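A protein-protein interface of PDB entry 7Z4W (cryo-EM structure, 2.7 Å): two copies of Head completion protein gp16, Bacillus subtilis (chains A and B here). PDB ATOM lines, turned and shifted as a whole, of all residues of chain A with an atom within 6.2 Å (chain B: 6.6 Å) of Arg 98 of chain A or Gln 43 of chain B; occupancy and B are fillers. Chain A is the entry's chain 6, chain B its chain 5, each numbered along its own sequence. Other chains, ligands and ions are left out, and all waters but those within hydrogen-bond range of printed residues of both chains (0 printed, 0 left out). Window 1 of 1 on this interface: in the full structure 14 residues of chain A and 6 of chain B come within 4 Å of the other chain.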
ATOM      1  N   ILE A  41      -3.483  21.298  17.072  1.00  0.00           N
ATOM      2  CA  ILE A  41      -3.216  21.279  18.506  1.00  0.00           C
ATOM      3  C   ILE A  41      -4.526  21.157  19.279  1.00  0.00           C
ATOM      4  O   ILE A  41      -5.611  21.495  18.791  1.00  0.00           O
ATOM      5  CB  ILE A  41      -2.418  22.517  18.942  1.00  0.00           C
ATOM      6  CG1 ILE A  41      -3.218  23.796  18.705  1.00  0.00           C
ATOM      7  CG2 ILE A  41      -1.093  22.569  18.210  1.00  0.00           C
ATOM      8  CD1 ILE A  41      -2.556  25.027  19.256  1.00  0.00           C
ATOM      9  N   GLU A  45      -4.101  23.135  24.570  1.00  0.00           N
ATOM     10  CA  GLU A  45      -2.851  23.690  24.068  1.00  0.00           C
ATOM     11  C   GLU A  45      -3.068  25.001  23.311  1.00  0.00           C
ATOM     12  O   GLU A  45      -2.126  25.792  23.177  1.00  0.00           O
ATOM     13  CB  GLU A  45      -2.164  22.623  23.198  1.00  0.00           C
ATOM     14  CG  GLU A  45      -0.801  22.968  22.620  1.00  0.00           C
ATOM     15  CD  GLU A  45      -0.138  21.799  21.917  1.00  0.00           C
ATOM     16  OE1 GLU A  45       0.898  22.014  21.254  1.00  0.00           O
ATOM     17  OE2 GLU A  45      -0.651  20.667  22.030  1.00  0.00           O
ATOM     18  N   LYS A  48      -2.530  28.037  25.613  1.00  0.00           N
ATOM     19  CA  LYS A  48      -1.112  28.202  25.898  1.00  0.00           C
ATOM     20  C   LYS A  48      -0.367  28.755  24.692  1.00  0.00           C
ATOM     21  O   LYS A  48       0.566  29.550  24.847  1.00  0.00           O
ATOM     22  CB  LYS A  48      -0.509  26.869  26.335  1.00  0.00           C
ATOM     23  CG  LYS A  48      -1.072  26.346  27.637  1.00  0.00           C
ATOM     24  CD  LYS A  48      -0.285  25.165  28.155  1.00  0.00           C
ATOM     25  CE  LYS A  48      -0.658  23.897  27.426  1.00  0.00           C
ATOM     26  NZ  LYS A  48      -0.147  22.696  28.131  1.00  0.00           N
ATOM     27  N   ASN A  59       1.015  20.023  15.003  1.00  0.00           N
ATOM     28  CA  ASN A  59       2.062  19.076  15.365  1.00  0.00           C
ATOM     29  C   ASN A  59       2.149  18.010  14.281  1.00  0.00           C
ATOM     30  O   ASN A  59       1.133  17.423  13.899  1.00  0.00           O
ATOM     31  CB  ASN A  59       1.776  18.418  16.718  1.00  0.00           C
ATOM     32  CG  ASN A  59       2.029  19.344  17.887  1.00  0.00           C
ATOM     33  OD1 ASN A  59       3.015  20.076  17.914  1.00  0.00           O
ATOM     34  ND2 ASN A  59       1.137  19.314  18.863  1.00  0.00           N
ATOM     35  N   ILE A  60       3.356  17.752  13.793  1.00  0.00           N
ATOM     36  CA  ILE A  60       3.594  16.788  12.728  1.00  0.00           C
ATOM     37  C   ILE A  60       4.448  15.670  13.302  1.00  0.00           C
ATOM     38  O   ILE A  60       5.549  15.923  13.803  1.00  0.00           O
ATOM     39  CB  ILE A  60       4.284  17.434  11.515  1.00  0.00           C
ATOM     40  CG1 ILE A  60       3.485  18.640  11.022  1.00  0.00           C
ATOM     41  CG2 ILE A  60       4.463  16.424  10.408  1.00  0.00           C
ATOM     42  CD1 ILE A  60       4.171  19.421   9.934  1.00  0.00           C
ATOM     43  N   TYR A  61       3.946  14.441  13.233  1.00  0.00           N
ATOM     44  CA  TYR A  61       4.674  13.271  13.700  1.00  0.00           C
ATOM     45  C   TYR A  61       5.120  12.455  12.497  1.00  0.00           C
ATOM     46  O   TYR A  61       4.321  12.182  11.598  1.00  0.00           O
ATOM     47  CB  TYR A  61       3.815  12.424  14.641  1.00  0.00           C
ATOM     48  CG  TYR A  61       3.527  13.110  15.954  1.00  0.00           C
ATOM     49  CD1 TYR A  61       4.398  12.984  17.028  1.00  0.00           C
ATOM     50  CD2 TYR A  61       2.395  13.898  16.113  1.00  0.00           C
ATOM     51  CE1 TYR A  61       4.145  13.618  18.227  1.00  0.00           C
ATOM     52  CE2 TYR A  61       2.135  14.537  17.306  1.00  0.00           C
ATOM     53  CZ  TYR A  61       3.011  14.392  18.359  1.00  0.00           C
ATOM     54  OH  TYR A  61       2.753  15.024  19.551  1.00  0.00           O
ATOM     55  N   THR A  62       6.392  12.085  12.476  1.00  0.00           N
ATOM     56  CA  THR A  62       6.962  11.363  11.350  1.00  0.00           C
ATOM     57  C   THR A  62       7.997  10.397  11.904  1.00  0.00           C
ATOM     58  O   THR A  62       8.448  10.564  13.040  1.00  0.00           O
ATOM     59  CB  THR A  62       7.569  12.343  10.326  1.00  0.00           C
ATOM     60  OG1 THR A  62       7.850  11.674   9.095  1.00  0.00           O
ATOM     61  CG2 THR A  62       8.840  12.992  10.848  1.00  0.00           C
ATOM     62  N   ASP A  86      12.924  24.227  16.426  1.00  0.00           N
ATOM     63  CA  ASP A  86      13.775  23.119  16.021  1.00  0.00           C
ATOM     64  C   ASP A  86      13.016  21.797  16.085  1.00  0.00           C
ATOM     65  O   ASP A  86      12.158  21.621  16.957  1.00  0.00           O
ATOM     66  CB  ASP A  86      15.007  23.048  16.923  1.00  0.00           C
ATOM     67  CG  ASP A  86      16.182  22.371  16.256  1.00  0.00           C
ATOM     68  OD1 ASP A  86      16.171  21.130  16.140  1.00  0.00           O
ATOM     69  OD2 ASP A  86      17.131  23.080  15.859  1.00  0.00           O
ATOM     70  N   PRO A  87      13.276  20.878  15.151  1.00  0.00           N
ATOM     71  CA  PRO A  87      12.681  19.536  15.241  1.00  0.00           C
ATOM     72  C   PRO A  87      13.156  18.779  16.474  1.00  0.00           C
ATOM     73  O   PRO A  87      14.307  18.896  16.897  1.00  0.00           O
ATOM     74  CB  PRO A  87      13.153  18.855  13.953  1.00  0.00           C
ATOM     75  CG  PRO A  87      13.387  19.969  13.004  1.00  0.00           C
ATOM     76  CD  PRO A  87      13.845  21.140  13.817  1.00  0.00           C
ATOM     77  N   VAL A  88      12.253  17.988  17.045  1.00  0.00           N
ATOM     78  CA  VAL A  88      12.484  17.296  18.307  1.00  0.00           C
ATOM     79  C   VAL A  88      12.402  15.795  18.067  1.00  0.00           C
ATOM     80  O   VAL A  88      11.403  15.300  17.535  1.00  0.00           O
ATOM     81  CB  VAL A  88      11.471  17.730  19.384  1.00  0.00           C
ATOM     82  CG1 VAL A  88      11.616  16.881  20.639  1.00  0.00           C
ATOM     83  CG2 VAL A  88      11.635  19.201  19.708  1.00  0.00           C
ATOM     84  N   ASP A  89      13.449  15.078  18.460  1.00  0.00           N
ATOM     85  CA  ASP A  89      13.425  13.624  18.503  1.00  0.00           C
ATOM     86  C   ASP A  89      12.943  13.195  19.885  1.00  0.00           C
ATOM     87  O   ASP A  89      13.533  13.586  20.895  1.00  0.00           O
ATOM     88  CB  ASP A  89      14.809  13.055  18.200  1.00  0.00           C
ATOM     89  CG  ASP A  89      14.903  11.580  18.491  1.00  0.00           C
ATOM     90  OD1 ASP A  89      13.953  10.844  18.147  1.00  0.00           O
ATOM     91  OD2 ASP A  89      15.924  11.155  19.063  1.00  0.00           O
ATOM     92  N   LEU A  90      11.880  12.390  19.921  1.00  0.00           N
ATOM     93  CA  LEU A  90      11.179  12.091  21.167  1.00  0.00           C
ATOM     94  C   LEU A  90      12.030  11.212  22.075  1.00  0.00           C
ATOM     95  O   LEU A  90      12.429  10.108  21.687  1.00  0.00           O
ATOM     96  CB  LEU A  90       9.844  11.412  20.872  1.00  0.00           C
ATOM     97  CG  LEU A  90       8.801  12.182  20.055  1.00  0.00           C
ATOM     98  CD1 LEU A  90       7.458  11.484  20.130  1.00  0.00           C
ATOM     99  CD2 LEU A  90       8.683  13.623  20.514  1.00  0.00           C
ATOM    100  N   ILE A  96      10.827   8.628  16.538  1.00  0.00           N
ATOM    101  CA  ILE A  96       9.762   9.492  16.037  1.00  0.00           C
ATOM    102  C   ILE A  96      10.208  10.944  16.177  1.00  0.00           C
ATOM    103  O   ILE A  96      10.717  11.342  17.230  1.00  0.00           O
ATOM    104  CB  ILE A  96       8.431   9.253  16.786  1.00  0.00           C
ATOM    105  CG1 ILE A  96       7.941   7.814  16.601  1.00  0.00           C
ATOM    106  CG2 ILE A  96       7.339  10.203  16.310  1.00  0.00           C
ATOM    107  CD1 ILE A  96       6.667   7.490  17.344  1.00  0.00           C
ATOM    108  N   THR A  97      10.026  11.727  15.116  1.00  0.00           N
ATOM    109  CA  THR A  97      10.299  13.158  15.108  1.00  0.00           C
ATOM    110  C   THR A  97       8.984  13.931  15.162  1.00  0.00           C
ATOM    111  O   THR A  97       8.039  13.610  14.430  1.00  0.00           O
ATOM    112  CB  THR A  97      11.100  13.534  13.856  1.00  0.00           C
ATOM    113  OG1 THR A  97      12.366  12.872  13.886  1.00  0.00           O
ATOM    114  CG2 THR A  97      11.334  15.034  13.756  1.00  0.00           C
ATOM    115  N   ARG A  98       8.922  14.931  16.044  1.00  0.00           N
ATOM    116  CA  ARG A  98       7.807  15.869  16.126  1.00  0.00           C
ATOM    117  C   ARG A  98       8.263  17.251  15.667  1.00  0.00           C
ATOM    118  O   ARG A  98       9.307  17.740  16.105  1.00  0.00           O
ATOM    119  CB  ARG A  98       7.253  15.945  17.552  1.00  0.00           C
ATOM    120  CG  ARG A  98       6.107  16.940  17.718  1.00  0.00           C
ATOM    121  CD  ARG A  98       5.504  16.911  19.112  1.00  0.00           C
ATOM    122  NE  ARG A  98       6.475  17.269  20.139  1.00  0.00           N
ATOM    123  CZ  ARG A  98       6.580  16.658  21.314  1.00  0.00           C
ATOM    124  NH1 ARG A  98       5.771  15.656  21.620  1.00  0.00           N
ATOM    125  NH2 ARG A  98       7.500  17.052  22.182  1.00  0.00           N
ATOM    126  N   ILE A  99       7.481  17.868  14.780  1.00  0.00           N
ATOM    127  CA  ILE A  99       7.737  19.216  14.278  1.00  0.00           C
ATOM    128  C   ILE A  99       6.525  20.087  14.579  1.00  0.00           C
ATOM    129  O   ILE A  99       5.385  19.672  14.353  1.00  0.00           O
ATOM    130  CB  ILE A  99       8.034  19.224  12.760  1.00  0.00           C
ATOM    131  CG1 ILE A  99       8.991  18.099  12.368  1.00  0.00           C
ATOM    132  CG2 ILE A  99       8.611  20.561  12.329  1.00  0.00           C
ATOM    133  CD1 ILE A  99       8.960  17.770  10.899  1.00  0.00           C
ATOM    134  N   LYS A 100       6.762  21.295  15.077  1.00  0.00           N
ATOM    135  CA  LYS A 100       5.700  22.273  15.275  1.00  0.00           C
ATOM    136  C   LYS A 100       5.657  23.232  14.092  1.00  0.00           C
ATOM    137  O   LYS A 100       6.700  23.637  13.575  1.00  0.00           O
ATOM    138  CB  LYS A 100       5.904  23.048  16.577  1.00  0.00           C
ATOM    139  CG  LYS A 100       6.065  22.165  17.801  1.00  0.00           C
ATOM    140  CD  LYS A 100       6.357  22.976  19.047  1.00  0.00           C
ATOM    141  CE  LYS A 100       7.754  23.578  19.008  1.00  0.00           C
ATOM    142  NZ  LYS A 100       8.816  22.598  19.364  1.00  0.00           N
ATOM    143  N   ILE B  41      12.968  18.336  26.472  1.00  0.00           N
ATOM    144  CA  ILE B  41      11.895  18.605  27.420  1.00  0.00           C
ATOM    145  C   ILE B  41      10.548  18.259  26.794  1.00  0.00           C
ATOM    146  O   ILE B  41      10.387  18.208  25.569  1.00  0.00           O
ATOM    147  CB  ILE B  41      11.933  20.062  27.908  1.00  0.00           C
ATOM    148  CG1 ILE B  41      11.683  21.033  26.758  1.00  0.00           C
ATOM    149  CG2 ILE B  41      13.263  20.356  28.573  1.00  0.00           C
ATOM    150  CD1 ILE B  41      11.551  22.463  27.199  1.00  0.00           C
ATOM    151  N   SER B  42       9.572  17.994  27.656  1.00  0.00           N
ATOM    152  CA  SER B  42       8.287  17.489  27.204  1.00  0.00           C
ATOM    153  C   SER B  42       7.466  18.600  26.551  1.00  0.00           C
ATOM    154  O   SER B  42       7.829  19.779  26.571  1.00  0.00           O
ATOM    155  CB  SER B  42       7.519  16.861  28.366  1.00  0.00           C
ATOM    156  OG  SER B  42       7.155  17.827  29.330  1.00  0.00           O
ATOM    157  N   GLN B  43       6.344  18.194  25.950  1.00  0.00           N
ATOM    158  CA  GLN B  43       5.450  19.129  25.276  1.00  0.00           C
ATOM    159  C   GLN B  43       4.809  20.110  26.249  1.00  0.00           C
ATOM    160  O   GLN B  43       4.500  21.243  25.870  1.00  0.00           O
ATOM    161  CB  GLN B  43       4.369  18.354  24.523  1.00  0.00           C
ATOM    162  CG  GLN B  43       3.459  19.203  23.664  1.00  0.00           C
ATOM    163  CD  GLN B  43       2.523  18.369  22.816  1.00  0.00           C
ATOM    164  OE1 GLN B  43       2.612  17.144  22.798  1.00  0.00           O
ATOM    165  NE2 GLN B  43       1.620  19.030  22.106  1.00  0.00           N
ATOM    166  N   GLU B  44       4.611  19.698  27.500  1.00  0.00           N
ATOM    167  CA  GLU B  44       4.033  20.577  28.508  1.00  0.00           C
ATOM    168  C   GLU B  44       5.076  21.525  29.087  1.00  0.00           C
ATOM    169  O   GLU B  44       4.767  22.680  29.396  1.00  0.00           O
ATOM    170  CB  GLU B  44       3.388  19.740  29.615  1.00  0.00           C
ATOM    171  CG  GLU B  44       2.136  18.976  29.180  1.00  0.00           C
ATOM    172  CD  GLU B  44       2.437  17.641  28.500  1.00  0.00           C
ATOM    173  OE1 GLU B  44       3.622  17.251  28.425  1.00  0.00           O
ATOM    174  OE2 GLU B  44       1.482  16.989  28.024  1.00  0.00           O
ATOM    175  N   GLU B  45       6.313  21.054  29.227  1.00  0.00           N
ATOM    176  CA  GLU B  45       7.403  21.845  29.781  1.00  0.00           C
ATOM    177  C   GLU B  45       7.892  22.916  28.805  1.00  0.00           C
ATOM    178  O   GLU B  45       8.498  23.904  29.236  1.00  0.00           O
ATOM    179  CB  GLU B  45       8.528  20.881  30.198  1.00  0.00           C
ATOM    180  CG  GLU B  45       9.775  21.481  30.824  1.00  0.00           C
ATOM    181  CD  GLU B  45      10.640  20.449  31.518  1.00  0.00           C
ATOM    182  OE1 GLU B  45      11.776  20.790  31.909  1.00  0.00           O
ATOM    183  OE2 GLU B  45      10.186  19.297  31.675  1.00  0.00           O
ATOM    184  N   TYR B  46       7.580  22.767  27.512  1.00  0.00           N
ATOM    185  CA  TYR B  46       8.004  23.724  26.491  1.00  0.00           C
ATOM    186  C   TYR B  46       7.367  25.094  26.707  1.00  0.00           C
ATOM    187  O   TYR B  46       8.045  26.126  26.638  1.00  0.00           O
ATOM    188  CB  TYR B  46       7.651  23.169  25.105  1.00  0.00           C
ATOM    189  CG  TYR B  46       7.933  24.091  23.938  1.00  0.00           C
ATOM    190  CD1 TYR B  46       9.207  24.187  23.398  1.00  0.00           C
ATOM    191  CD2 TYR B  46       6.919  24.851  23.363  1.00  0.00           C
ATOM    192  CE1 TYR B  46       9.468  25.023  22.330  1.00  0.00           C
ATOM    193  CE2 TYR B  46       7.171  25.692  22.301  1.00  0.00           C
ATOM    194  CZ  TYR B  46       8.447  25.771  21.787  1.00  0.00           C
ATOM    195  OH  TYR B  46       8.704  26.603  20.729  1.00  0.00           O
ATOM    196  N   TYR B  47       6.061  25.117  26.987  1.00  0.00           N
ATOM    197  CA  TYR B  47       5.356  26.379  27.182  1.00  0.00           C
ATOM    198  C   TYR B  47       5.757  27.057  28.483  1.00  0.00           C
ATOM    199  O   TYR B  47       5.715  28.288  28.574  1.00  0.00           O
ATOM    200  CB  TYR B  47       3.848  26.143  27.147  1.00  0.00           C
ATOM    201  CG  TYR B  47       3.343  25.738  25.786  1.00  0.00           C
ATOM    202  CD1 TYR B  47       3.148  26.685  24.790  1.00  0.00           C
ATOM    203  CD2 TYR B  47       3.071  24.406  25.492  1.00  0.00           C
ATOM    204  CE1 TYR B  47       2.691  26.322  23.543  1.00  0.00           C
ATOM    205  CE2 TYR B  47       2.614  24.032  24.247  1.00  0.00           C
ATOM    206  CZ  TYR B  47       2.426  24.995  23.277  1.00  0.00           C
ATOM    207  OH  TYR B  47       1.973  24.633  22.033  1.00  0.00           O
ATOM    208  N   LYS B  48       6.157  26.281  29.490  1.00  0.00           N
ATOM    209  CA  LYS B  48       6.669  26.867  30.720  1.00  0.00           C
ATOM    210  C   LYS B  48       8.076  27.416  30.526  1.00  0.00           C
ATOM    211  O   LYS B  48       8.426  28.448  31.106  1.00  0.00           O
ATOM    212  CB  LYS B  48       6.649  25.833  31.844  1.00  0.00           C
ATOM    213  CG  LYS B  48       5.258  25.390  32.242  1.00  0.00           C
ATOM    214  CD  LYS B  48       5.270  24.572  33.513  1.00  0.00           C
ATOM    215  CE  LYS B  48       5.699  23.150  33.242  1.00  0.00           C
ATOM    216  NZ  LYS B  48       5.410  22.263  34.397  1.00  0.00           N
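The side-chain amide nitrogen (NE2) of Gln 43 of chain B lies within hydrogen-bond range of the side-chain carboxylate (OE2) of Glu 45 of chain A, 2.8 Å away. The side-chain amide nitrogen of Gln 43 of chain B sits close to the side-chain amide nitrogen of Asn 59 of chain A, 3.3 Å away. OE1 of Glu 45 of chain A sits at hydrogen-bond distance from OH of Tyr 47 of chain B, at 2.9 Å.
3 positions are printed for both chains. Of the 7 pairs that touch across the chains among the printed residues, none has its exchanged pair printed and touching as well.
Of the printed residues of chain B, Glu 45 of chain A touches Gln 43 and Tyr 47. Printed residues of chain B within 4 Å of Asn 59 of chain A: Gln 43. Ile 96 of chain A touches none of the printed residues of chain B. Ile 99 of chain A touches none of the printed residues of chain B. Gln 43 of chain B touches just these residues of chain A: Glu 45 (2.8 Å), Asn 59 (3.3 Å), Tyr 61 (3.9 Å) and Arg 98 (3.7 Å). Of the printed residues of chain A, Tyr 46 of chain B touches Lys 100. The nearest residue of chain B that does not touch Arg 98 of chain A is Ile 41 of chain B (4.6 Å). The nearest residue of chain A that does not touch Gln 43 of chain B is Lys 48 of chain A (5.4 Å).
Among the printed residues, merely in contact across the chains: Lys 48 of chain A with Tyr 47 of chain B, Tyr 61 of chain A with Gln 43 of chain B, Arg 98 of chain A with Gln 43 of chain B and Lys 100 of chain A with Tyr 46 of chain B.
Printed residues of chain A that touch a printed residue of chain B: Glu 45, Lys 48, Asn 59, Tyr 61, Arg 98 and Lys 100. Hydrophobic or aromatic side chains of chain A within 4 Å of the printed part of chain B: Tyr 61. Printed residues of chain B that touch a printed residue of chain A: Gln 43, Tyr 46 and Tyr 47. Hydrophobic or aromatic side chains of chain B within 4 Å of the printed part of chain A: Tyr 46 and Tyr 47. Among the printed residues, 7 pairs touch across the chains. Among the printed residues, no Asp or Glu carboxylate lies within 4 Å of a Lys or Arg side-chain nitrogen of the other chain.
The backbone carbonyl oxygen (O) of Val 88 of chain A lies within hydrogen-bond range of the backbone NH (N) of Arg 98 of chain A (2.9 Å).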
